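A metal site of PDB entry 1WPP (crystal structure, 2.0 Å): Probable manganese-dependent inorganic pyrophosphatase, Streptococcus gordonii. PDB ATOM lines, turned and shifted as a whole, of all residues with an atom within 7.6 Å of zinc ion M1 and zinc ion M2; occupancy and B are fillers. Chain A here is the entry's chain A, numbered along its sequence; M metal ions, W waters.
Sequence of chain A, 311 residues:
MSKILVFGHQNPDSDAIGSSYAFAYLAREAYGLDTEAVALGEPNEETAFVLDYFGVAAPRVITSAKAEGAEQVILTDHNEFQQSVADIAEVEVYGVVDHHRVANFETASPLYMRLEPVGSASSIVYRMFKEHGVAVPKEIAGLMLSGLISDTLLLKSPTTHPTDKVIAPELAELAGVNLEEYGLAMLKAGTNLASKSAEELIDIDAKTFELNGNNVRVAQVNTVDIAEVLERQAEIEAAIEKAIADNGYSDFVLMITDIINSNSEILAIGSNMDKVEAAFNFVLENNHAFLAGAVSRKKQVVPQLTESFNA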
ATOM      1  N   GLY A   8       8.428 -24.074   3.926  1.00  0.00           N
ATOM      2  CA  GLY A   8       8.619 -22.640   3.715  1.00  0.00           C
ATOM      3  C   GLY A   8       7.553 -22.052   2.760  1.00  0.00           C
ATOM      4  O   GLY A   8       6.605 -22.759   2.387  1.00  0.00           O
ATOM      5  N   HIS A   9       7.758 -20.801   2.333  1.00  0.00           N
ATOM      6  CA  HIS A   9       6.757 -20.051   1.567  1.00  0.00           C
ATOM      7  C   HIS A   9       6.644 -20.531   0.140  1.00  0.00           C
ATOM      8  O   HIS A   9       7.507 -21.297  -0.343  1.00  0.00           O
ATOM      9  CB  HIS A   9       7.045 -18.521   1.578  1.00  0.00           C
ATOM     10  CG  HIS A   9       8.494 -18.161   1.332  1.00  0.00           C
ATOM     11  ND1 HIS A   9       9.041 -18.076   0.075  1.00  0.00           N
ATOM     12  CD2 HIS A   9       9.486 -17.825   2.193  1.00  0.00           C
ATOM     13  CE1 HIS A   9      10.326 -17.717   0.172  1.00  0.00           C
ATOM     14  NE2 HIS A   9      10.617 -17.556   1.455  1.00  0.00           N
ATOM     15  N   GLN A  10       5.568 -20.100  -0.517  1.00  0.00           N
ATOM     16  CA  GLN A  10       5.446 -20.182  -1.955  1.00  0.00           C
ATOM     17  C   GLN A  10       6.609 -19.451  -2.599  1.00  0.00           C
ATOM     18  O   GLN A  10       7.176 -18.509  -2.009  1.00  0.00           O
ATOM     19  CB  GLN A  10       4.138 -19.533  -2.454  1.00  0.00           C
ATOM     20  CG  GLN A  10       2.845 -20.146  -1.941  1.00  0.00           C
ATOM     21  CD  GLN A  10       2.382 -21.334  -2.763  1.00  0.00           C
ATOM     22  OE1 GLN A  10       3.063 -21.749  -3.690  1.00  0.00           O
ATOM     23  NE2 GLN A  10       1.238 -21.877  -2.427  1.00  0.00           N
ATOM     24  N   ASN A  11       6.937 -19.873  -3.817  1.00  0.00           N
ATOM     25  CA  ASN A  11       8.167 -19.482  -4.492  1.00  0.00           C
ATOM     26  C   ASN A  11       9.351 -19.650  -3.574  1.00  0.00           C
ATOM     27  O   ASN A  11       9.963 -18.660  -3.202  1.00  0.00           O
ATOM     28  CB  ASN A  11       8.060 -18.051  -5.045  1.00  0.00           C
ATOM     29  CG  ASN A  11       6.863 -17.897  -5.979  1.00  0.00           C
ATOM     30  OD1 ASN A  11       6.681 -18.696  -6.911  1.00  0.00           O
ATOM     31  ND2 ASN A  11       6.038 -16.877  -5.720  1.00  0.00           N
ATOM     32  N   PRO A  12       9.632 -20.868  -3.117  1.00  0.00           N
ATOM     33  CA  PRO A  12      10.668 -21.052  -2.083  1.00  0.00           C
ATOM     34  C   PRO A  12      12.059 -20.515  -2.484  1.00  0.00           C
ATOM     35  O   PRO A  12      12.479 -20.609  -3.646  1.00  0.00           O
ATOM     36  CB  PRO A  12      10.659 -22.562  -1.864  1.00  0.00           C
ATOM     37  CG  PRO A  12      10.102 -23.073  -3.187  1.00  0.00           C
ATOM     38  CD  PRO A  12       9.005 -22.141  -3.499  1.00  0.00           C
ATOM     39  N   ASP A  13      12.739 -19.878  -1.534  1.00  0.00           N
ATOM     40  CA  ASP A  13      14.102 -19.427  -1.740  1.00  0.00           C
ATOM     41  C   ASP A  13      14.972 -20.435  -0.932  1.00  0.00           C
ATOM     42  O   ASP A  13      14.400 -21.328  -0.325  1.00  0.00           O
ATOM     43  CB  ASP A  13      14.241 -17.944  -1.296  1.00  0.00           C
ATOM     44  CG  ASP A  13      13.762 -17.710   0.141  1.00  0.00           C
ATOM     45  OD1 ASP A  13      13.466 -16.549   0.534  1.00  0.00           O
ATOM     46  OD2 ASP A  13      13.692 -18.636   0.983  1.00  0.00           O
ATOM     47  N   SER A  14      16.306 -20.285  -0.861  1.00  0.00           N
ATOM     48  CA  SER A  14      17.166 -21.269  -0.172  1.00  0.00           C
ATOM     49  C   SER A  14      16.884 -21.393   1.301  1.00  0.00           C
ATOM     50  O   SER A  14      17.016 -22.489   1.854  1.00  0.00           O
ATOM     51  CB  SER A  14      18.658 -20.935  -0.316  1.00  0.00           C
ATOM     52  OG  SER A  14      19.047 -21.036  -1.685  1.00  0.00           O
ATOM     53  N   ASP A  15      16.591 -20.253   1.945  1.00  0.00           N
ATOM     54  CA  ASP A  15      16.259 -20.231   3.360  1.00  0.00           C
ATOM     55  C   ASP A  15      14.974 -20.970   3.661  1.00  0.00           C
ATOM     56  O   ASP A  15      14.897 -21.652   4.672  1.00  0.00           O
ATOM     57  CB  ASP A  15      16.191 -18.799   3.894  1.00  0.00           C
ATOM     58  CG  ASP A  15      16.016 -18.732   5.396  1.00  0.00           C
ATOM     59  OD1 ASP A  15      16.697 -19.518   6.081  1.00  0.00           O
ATOM     60  OD2 ASP A  15      15.201 -17.939   5.980  1.00  0.00           O
ATOM     61  N   ALA A  16      13.970 -20.840   2.793  1.00  0.00           N
ATOM     62  CA  ALA A  16      12.680 -21.532   2.964  1.00  0.00           C
ATOM     63  C   ALA A  16      12.882 -23.081   2.945  1.00  0.00           C
ATOM     64  O   ALA A  16      12.421 -23.821   3.856  1.00  0.00           O
ATOM     65  CB  ALA A  16      11.652 -21.058   1.846  1.00  0.00           C
ATOM     66  N   ILE A  17      13.635 -23.564   1.958  1.00  0.00           N
ATOM     67  CA  ILE A  17      13.847 -25.024   1.781  1.00  0.00           C
ATOM     68  C   ILE A  17      14.810 -25.469   2.909  1.00  0.00           C
ATOM     69  O   ILE A  17      14.578 -26.480   3.585  1.00  0.00           O
ATOM     70  CB  ILE A  17      14.488 -25.293   0.361  1.00  0.00           C
ATOM     71  CG1 ILE A  17      13.523 -25.010  -0.791  1.00  0.00           C
ATOM     72  CG2 ILE A  17      15.129 -26.704   0.218  1.00  0.00           C
ATOM     73  CD1 ILE A  17      12.386 -25.822  -0.813  1.00  0.00           C
ATOM     74  N   SER A  19      15.553 -24.107   5.906  1.00  0.00           N
ATOM     75  CA  SER A  19      14.928 -24.065   7.226  1.00  0.00           C
ATOM     76  C   SER A  19      13.905 -25.168   7.485  1.00  0.00           C
ATOM     77  O   SER A  19      13.842 -25.731   8.619  1.00  0.00           O
ATOM     78  CB  SER A  19      14.362 -22.666   7.566  1.00  0.00           C
ATOM     79  OG  SER A  19      13.229 -22.350   6.754  1.00  0.00           O
ATOM     80  N   THR A  76       7.900 -22.456   8.203  1.00  0.00           N
ATOM     81  CA  THR A  76       9.220 -21.880   8.505  1.00  0.00           C
ATOM     82  C   THR A  76       9.465 -20.789   7.515  1.00  0.00           C
ATOM     83  O   THR A  76       8.894 -20.838   6.419  1.00  0.00           O
ATOM     84  CB  THR A  76      10.380 -22.900   8.495  1.00  0.00           C
ATOM     85  OG1 THR A  76      10.626 -23.421   7.163  1.00  0.00           O
ATOM     86  CG2 THR A  76      10.081 -24.155   9.414  1.00  0.00           C
ATOM     87  N   ASP A  77      10.250 -19.759   7.894  1.00  0.00           N
ATOM     88  CA  ASP A  77      10.570 -18.639   6.984  1.00  0.00           C
ATOM     89  C   ASP A  77       9.324 -17.878   6.442  1.00  0.00           C
ATOM     90  O   ASP A  77       9.437 -17.090   5.497  1.00  0.00           O
ATOM     91  CB  ASP A  77      11.446 -19.137   5.803  1.00  0.00           C
ATOM     92  CG  ASP A  77      12.144 -18.006   5.028  1.00  0.00           C
ATOM     93  OD1 ASP A  77      12.312 -18.170   3.788  1.00  0.00           O
ATOM     94  OD2 ASP A  77      12.590 -16.953   5.559  1.00  0.00           O
ATOM     95  N   HIS A  78       8.181 -18.022   7.075  1.00  0.00           N
ATOM     96  CA  HIS A  78       7.002 -17.199   6.707  1.00  0.00           C
ATOM     97  C   HIS A  78       5.894 -17.384   7.743  1.00  0.00           C
ATOM     98  O   HIS A  78       5.916 -18.355   8.534  1.00  0.00           O
ATOM     99  CB  HIS A  78       6.453 -17.566   5.309  1.00  0.00           C
ATOM    100  CG  HIS A  78       5.727 -18.870   5.262  1.00  0.00           C
ATOM    101  ND1 HIS A  78       6.358 -20.084   5.435  1.00  0.00           N
ATOM    102  CD2 HIS A  78       4.410 -19.159   5.041  1.00  0.00           C
ATOM    103  CE1 HIS A  78       5.471 -21.065   5.316  1.00  0.00           C
ATOM    104  NE2 HIS A  78       4.287 -20.529   5.080  1.00  0.00           N
ATOM    105  N   GLN A  83       1.323 -16.197   1.659  1.00  0.00           N
ATOM    106  CA  GLN A  83       2.602 -16.798   1.285  1.00  0.00           C
ATOM    107  C   GLN A  83       2.609 -18.285   1.522  1.00  0.00           C
ATOM    108  O   GLN A  83       3.613 -18.946   1.216  1.00  0.00           O
ATOM    109  CB  GLN A  83       3.764 -16.184   2.077  1.00  0.00           C
ATOM    110  CG  GLN A  83       3.961 -14.692   1.775  1.00  0.00           C
ATOM    111  CD  GLN A  83       5.023 -14.073   2.684  1.00  0.00           C
ATOM    112  OE1 GLN A  83       5.623 -14.783   3.480  1.00  0.00           O
ATOM    113  NE2 GLN A  83       5.254 -12.786   2.572  1.00  0.00           N
ATOM    114  N   ASP A  98      10.253 -18.096  12.201  1.00  0.00           N
ATOM    115  CA  ASP A  98      10.385 -17.128  11.129  1.00  0.00           C
ATOM    116  C   ASP A  98      11.257 -15.945  11.552  1.00  0.00           C
ATOM    117  O   ASP A  98      11.617 -15.855  12.728  1.00  0.00           O
ATOM    118  CB  ASP A  98       8.965 -16.687  10.712  1.00  0.00           C
ATOM    119  CG  ASP A  98       8.952 -15.925   9.413  1.00  0.00           C
ATOM    120  OD1 ASP A  98       7.948 -15.216   9.166  1.00  0.00           O
ATOM    121  OD2 ASP A  98       9.900 -15.969   8.594  1.00  0.00           O
ATOM    122  N   HIS A  99      11.577 -15.052  10.592  1.00  0.00           N
ATOM    123  CA  HIS A  99      12.372 -13.836  10.771  1.00  0.00           C
ATOM    124  C   HIS A  99      11.758 -12.594  10.041  1.00  0.00           C
ATOM    125  O   HIS A  99      12.448 -11.618   9.747  1.00  0.00           O
ATOM    126  CB  HIS A  99      13.834 -14.072  10.373  1.00  0.00           C
ATOM    127  CG  HIS A  99      14.070 -14.283   8.890  1.00  0.00           C
ATOM    128  ND1 HIS A  99      14.822 -13.405   8.128  1.00  0.00           N
ATOM    129  CD2 HIS A  99      13.754 -15.305   8.063  1.00  0.00           C
ATOM    130  CE1 HIS A  99      14.898 -13.848   6.884  1.00  0.00           C
ATOM    131  NE2 HIS A  99      14.270 -15.017   6.820  1.00  0.00           N
ATOM    132  N   HIS A 100      10.474 -12.663   9.754  1.00  0.00           N
ATOM    133  CA  HIS A 100       9.777 -11.545   9.070  1.00  0.00           C
ATOM    134  C   HIS A 100       8.803 -10.870  10.010  1.00  0.00           C
ATOM    135  O   HIS A 100       8.518 -11.366  11.104  1.00  0.00           O
ATOM    136  CB  HIS A 100       9.053 -12.078   7.821  1.00  0.00           C
ATOM    137  CG  HIS A 100       9.989 -12.645   6.809  1.00  0.00           C
ATOM    138  ND1 HIS A 100      10.343 -13.977   6.806  1.00  0.00           N
ATOM    139  CD2 HIS A 100      10.677 -12.071   5.778  1.00  0.00           C
ATOM    140  CE1 HIS A 100      11.189 -14.190   5.813  1.00  0.00           C
ATOM    141  NE2 HIS A 100      11.390 -13.056   5.157  1.00  0.00           N
ATOM    142  N   VAL A 118      16.470 -11.707  12.841  1.00  0.00           N
ATOM    143  CA  VAL A 118      17.850 -12.020  12.463  1.00  0.00           C
ATOM    144  C   VAL A 118      17.870 -12.271  10.963  1.00  0.00           C
ATOM    145  O   VAL A 118      16.885 -12.001  10.275  1.00  0.00           O
ATOM    146  CB  VAL A 118      18.421 -13.253  13.260  1.00  0.00           C
ATOM    147  CG1 VAL A 118      18.467 -12.958  14.779  1.00  0.00           C
ATOM    148  CG2 VAL A 118      17.599 -14.544  13.005  1.00  0.00           C
ATOM    149  N   GLY A 119      18.983 -12.791  10.443  1.00  0.00           N
ATOM    150  CA  GLY A 119      19.231 -12.780   9.005  1.00  0.00           C
ATOM    151  C   GLY A 119      18.442 -13.817   8.210  1.00  0.00           C
ATOM    152  O   GLY A 119      18.212 -13.612   7.032  1.00  0.00           O
ATOM    153  N   SER A 120      18.018 -14.901   8.861  1.00  0.00           N
ATOM    154  CA  SER A 120      17.351 -15.986   8.142  1.00  0.00           C
ATOM    155  C   SER A 120      16.672 -16.865   9.166  1.00  0.00           C
ATOM    156  O   SER A 120      17.065 -16.904  10.357  1.00  0.00           O
ATOM    157  CB  SER A 120      18.364 -16.867   7.384  1.00  0.00           C
ATOM    158  OG  SER A 120      19.198 -17.569   8.342  1.00  0.00           O
ATOM    159  N   ALA A 121      15.682 -17.639   8.708  1.00  0.00           N
ATOM    160  CA  ALA A 121      15.042 -18.629   9.547  1.00  0.00           C
ATOM    161  C   ALA A 121      16.006 -19.767   9.862  1.00  0.00           C
ATOM    162  O   ALA A 121      15.941 -20.355  10.951  1.00  0.00           O
ATOM    163  CB  ALA A 121      13.769 -19.178   8.885  1.00  0.00           C
ATOM    164  N   SER A 122      16.928 -20.031   8.956  1.00  0.00           N
ATOM    165  CA  SER A 122      17.842 -21.139   9.165  1.00  0.00           C
ATOM    166  C   SER A 122      18.762 -20.860  10.375  1.00  0.00           C
ATOM    167  O   SER A 122      19.176 -21.803  11.083  1.00  0.00           O
ATOM    168  CB  SER A 122      18.684 -21.385   7.913  1.00  0.00           C
ATOM    169  OG  SER A 122      17.954 -22.020   6.892  1.00  0.00           O
ATOM    170  N   GLY A 147      20.998 -21.172   3.621  1.00  0.00           N
ATOM    171  CA  GLY A 147      19.877 -20.307   3.910  1.00  0.00           C
ATOM    172  C   GLY A 147      20.309 -18.937   4.399  1.00  0.00           C
ATOM    173  O   GLY A 147      19.821 -17.895   3.905  1.00  0.00           O
ATOM    174  N   LEU A 148      21.230 -18.942   5.361  1.00  0.00           N
ATOM    175  CA  LEU A 148      21.813 -17.734   5.917  1.00  0.00           C
ATOM    176  C   LEU A 148      22.609 -16.934   4.902  1.00  0.00           C
ATOM    177  O   LEU A 148      22.425 -15.698   4.796  1.00  0.00           O
ATOM    178  CB  LEU A 148      22.650 -18.061   7.164  1.00  0.00           C
ATOM    179  CG  LEU A 148      23.522 -16.904   7.746  1.00  0.00           C
ATOM    180  CD1 LEU A 148      22.675 -15.631   8.166  1.00  0.00           C
ATOM    181  CD2 LEU A 148      24.458 -17.434   8.857  1.00  0.00           C
ATOM    182  N   SER A 150      22.241 -17.021   1.586  1.00  0.00           N
ATOM    183  CA  SER A 150      21.295 -16.525   0.574  1.00  0.00           C
ATOM    184  C   SER A 150      20.511 -15.298   1.018  1.00  0.00           C
ATOM    185  O   SER A 150      20.448 -14.269   0.270  1.00  0.00           O
ATOM    186  CB  SER A 150      20.311 -17.653   0.203  1.00  0.00           C
ATOM    187  OG  SER A 150      19.224 -17.200  -0.552  1.00  0.00           O
ATOM    188  N   ASP A 151      19.934 -15.349   2.224  1.00  0.00           N
ATOM    189  CA  ASP A 151      19.102 -14.245   2.743  1.00  0.00           C
ATOM    190  C   ASP A 151      19.911 -12.939   3.012  1.00  0.00           C
ATOM    191  O   ASP A 151      19.364 -11.835   2.923  1.00  0.00           O
ATOM    192  CB  ASP A 151      18.333 -14.631   4.022  1.00  0.00           C
ATOM    193  CG  ASP A 151      16.957 -15.221   3.760  1.00  0.00           C
ATOM    194  OD1 ASP A 151      16.522 -15.374   2.561  1.00  0.00           O
ATOM    195  OD2 ASP A 151      16.236 -15.591   4.736  1.00  0.00           O
ATOM    196  N   ASP A 205      11.374 -12.444  -7.676  1.00  0.00           N
ATOM    197  CA  ASP A 205      11.267 -12.103  -6.272  1.00  0.00           C
ATOM    198  C   ASP A 205      10.685 -10.690  -6.166  1.00  0.00           C
ATOM    199  O   ASP A 205      11.414  -9.716  -6.092  1.00  0.00           O
ATOM    200  CB  ASP A 205      12.635 -12.202  -5.615  1.00  0.00           C
ATOM    201  CG  ASP A 205      12.618 -11.996  -4.121  1.00  0.00           C
ATOM    202  OD1 ASP A 205      11.598 -11.565  -3.536  1.00  0.00           O
ATOM    203  OD2 ASP A 205      13.624 -12.244  -3.424  1.00  0.00           O
ATOM    204  N   LYS A 298      13.863  -4.919   2.170  1.00  0.00           N
ATOM    205  CA  LYS A 298      13.038  -4.508   3.261  1.00  0.00           C
ATOM    206  C   LYS A 298      13.741  -3.464   4.125  1.00  0.00           C
ATOM    207  O   LYS A 298      13.076  -2.723   4.801  1.00  0.00           O
ATOM    208  CB  LYS A 298      12.548  -5.735   4.092  1.00  0.00           C
ATOM    209  CG  LYS A 298      13.411  -6.149   5.246  1.00  0.00           C
ATOM    210  CD  LYS A 298      12.796  -7.435   5.849  1.00  0.00           C
ATOM    211  CE  LYS A 298      13.837  -8.366   6.311  1.00  0.00           C
ATOM    212  NZ  LYS A 298      14.200  -9.483   5.331  1.00  0.00           N
HETATM  213 ZN    ZN M   1      14.420 -16.273   5.134  1.00  0.00          ZN
HETATM  214 ZN    ZN M   2      12.430 -16.852   2.267  1.00  0.00          ZN
HETATM  215  O   HOH W   1      11.042 -14.621   2.319  1.00  0.00           O
HETATM  216  O   HOH W   2      13.920 -15.887   3.312  1.00  0.00           O
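The backbone carbonyl oxygen (O) of Asp 77 sits close to a ring nitrogen (ND1) of His 100 (3.5 Å).
The backbone NH (N) of Ala 16 lies close to the side-chain carboxylate (OD1) of Asp 77 (3.3 Å).
The backbone NH (N) of Asp 15 sits close to the side-chain carboxylate (OD2) of Asp 13 (3.5 Å).
The side-chain carboxylate (OD1) of Asp 15 lies within hydrogen-bond range of the backbone NH (N) of Ala 121 (3.4 Å).
The side-chain carboxylate (OD1) of Asp 15 sits at hydrogen-bond distance from the side-chain hydroxyl (OG) of Ser 122 (2.9 Å).
The side-chain hydroxyl (OG) of Ser 19 is in hydrogen-bond range of the backbone carbonyl oxygen (O) of Asp 15, 2.8 Å away.
A ring nitrogen (ND1) of His 99 lies within hydrogen-bond range of the backbone carbonyl oxygen (O) of Val 118, at 3.3 Å.
A ring nitrogen (ND1) of His 100 lies within hydrogen-bond range of the side-chain carboxylate (OD2) of Asp 98 (2.7 Å).
CE1 of His 100 touches zinc ion M1 (3.9 Å).
Of the 29 residues printed, 5 come within 4 Å of zinc ion M1.
Along chain A the residues within 4 Å of zinc ion M1 span positions 15 to 151.
Water W2 binds zinc ion M1 (1.9 Å).
The side-chain carboxylate (OD2) of Asp 151 is bound to zinc ion M1 (2.0 Å).
OD2 of Asp 77 binds zinc ion M1 (2.0 Å).
Zinc ion M1 is bound by the side-chain carboxylate (OD2) of Asp 15 (2.0 Å).
NE2 of His 99 is bound to zinc ion M1, 2.1 Å away.
The side-chain carboxylate (OD1) of Asp 77 is bound to zinc ion M2 (2.0 Å).
Zinc ion M2 is bound by the side-chain carboxylate (OD1) of Asp 13, 2.0 Å away.
Water W2 is bound to zinc ion M2, 2.1 Å away.
A ring nitrogen (NE2) of His 9 binds zinc ion M2 (2.1 Å).
OD2 of Asp 13 binds zinc ion M2 (2.5 Å).
Slightly farther from zinc ion M2 lies water W1 (2.6 Å).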
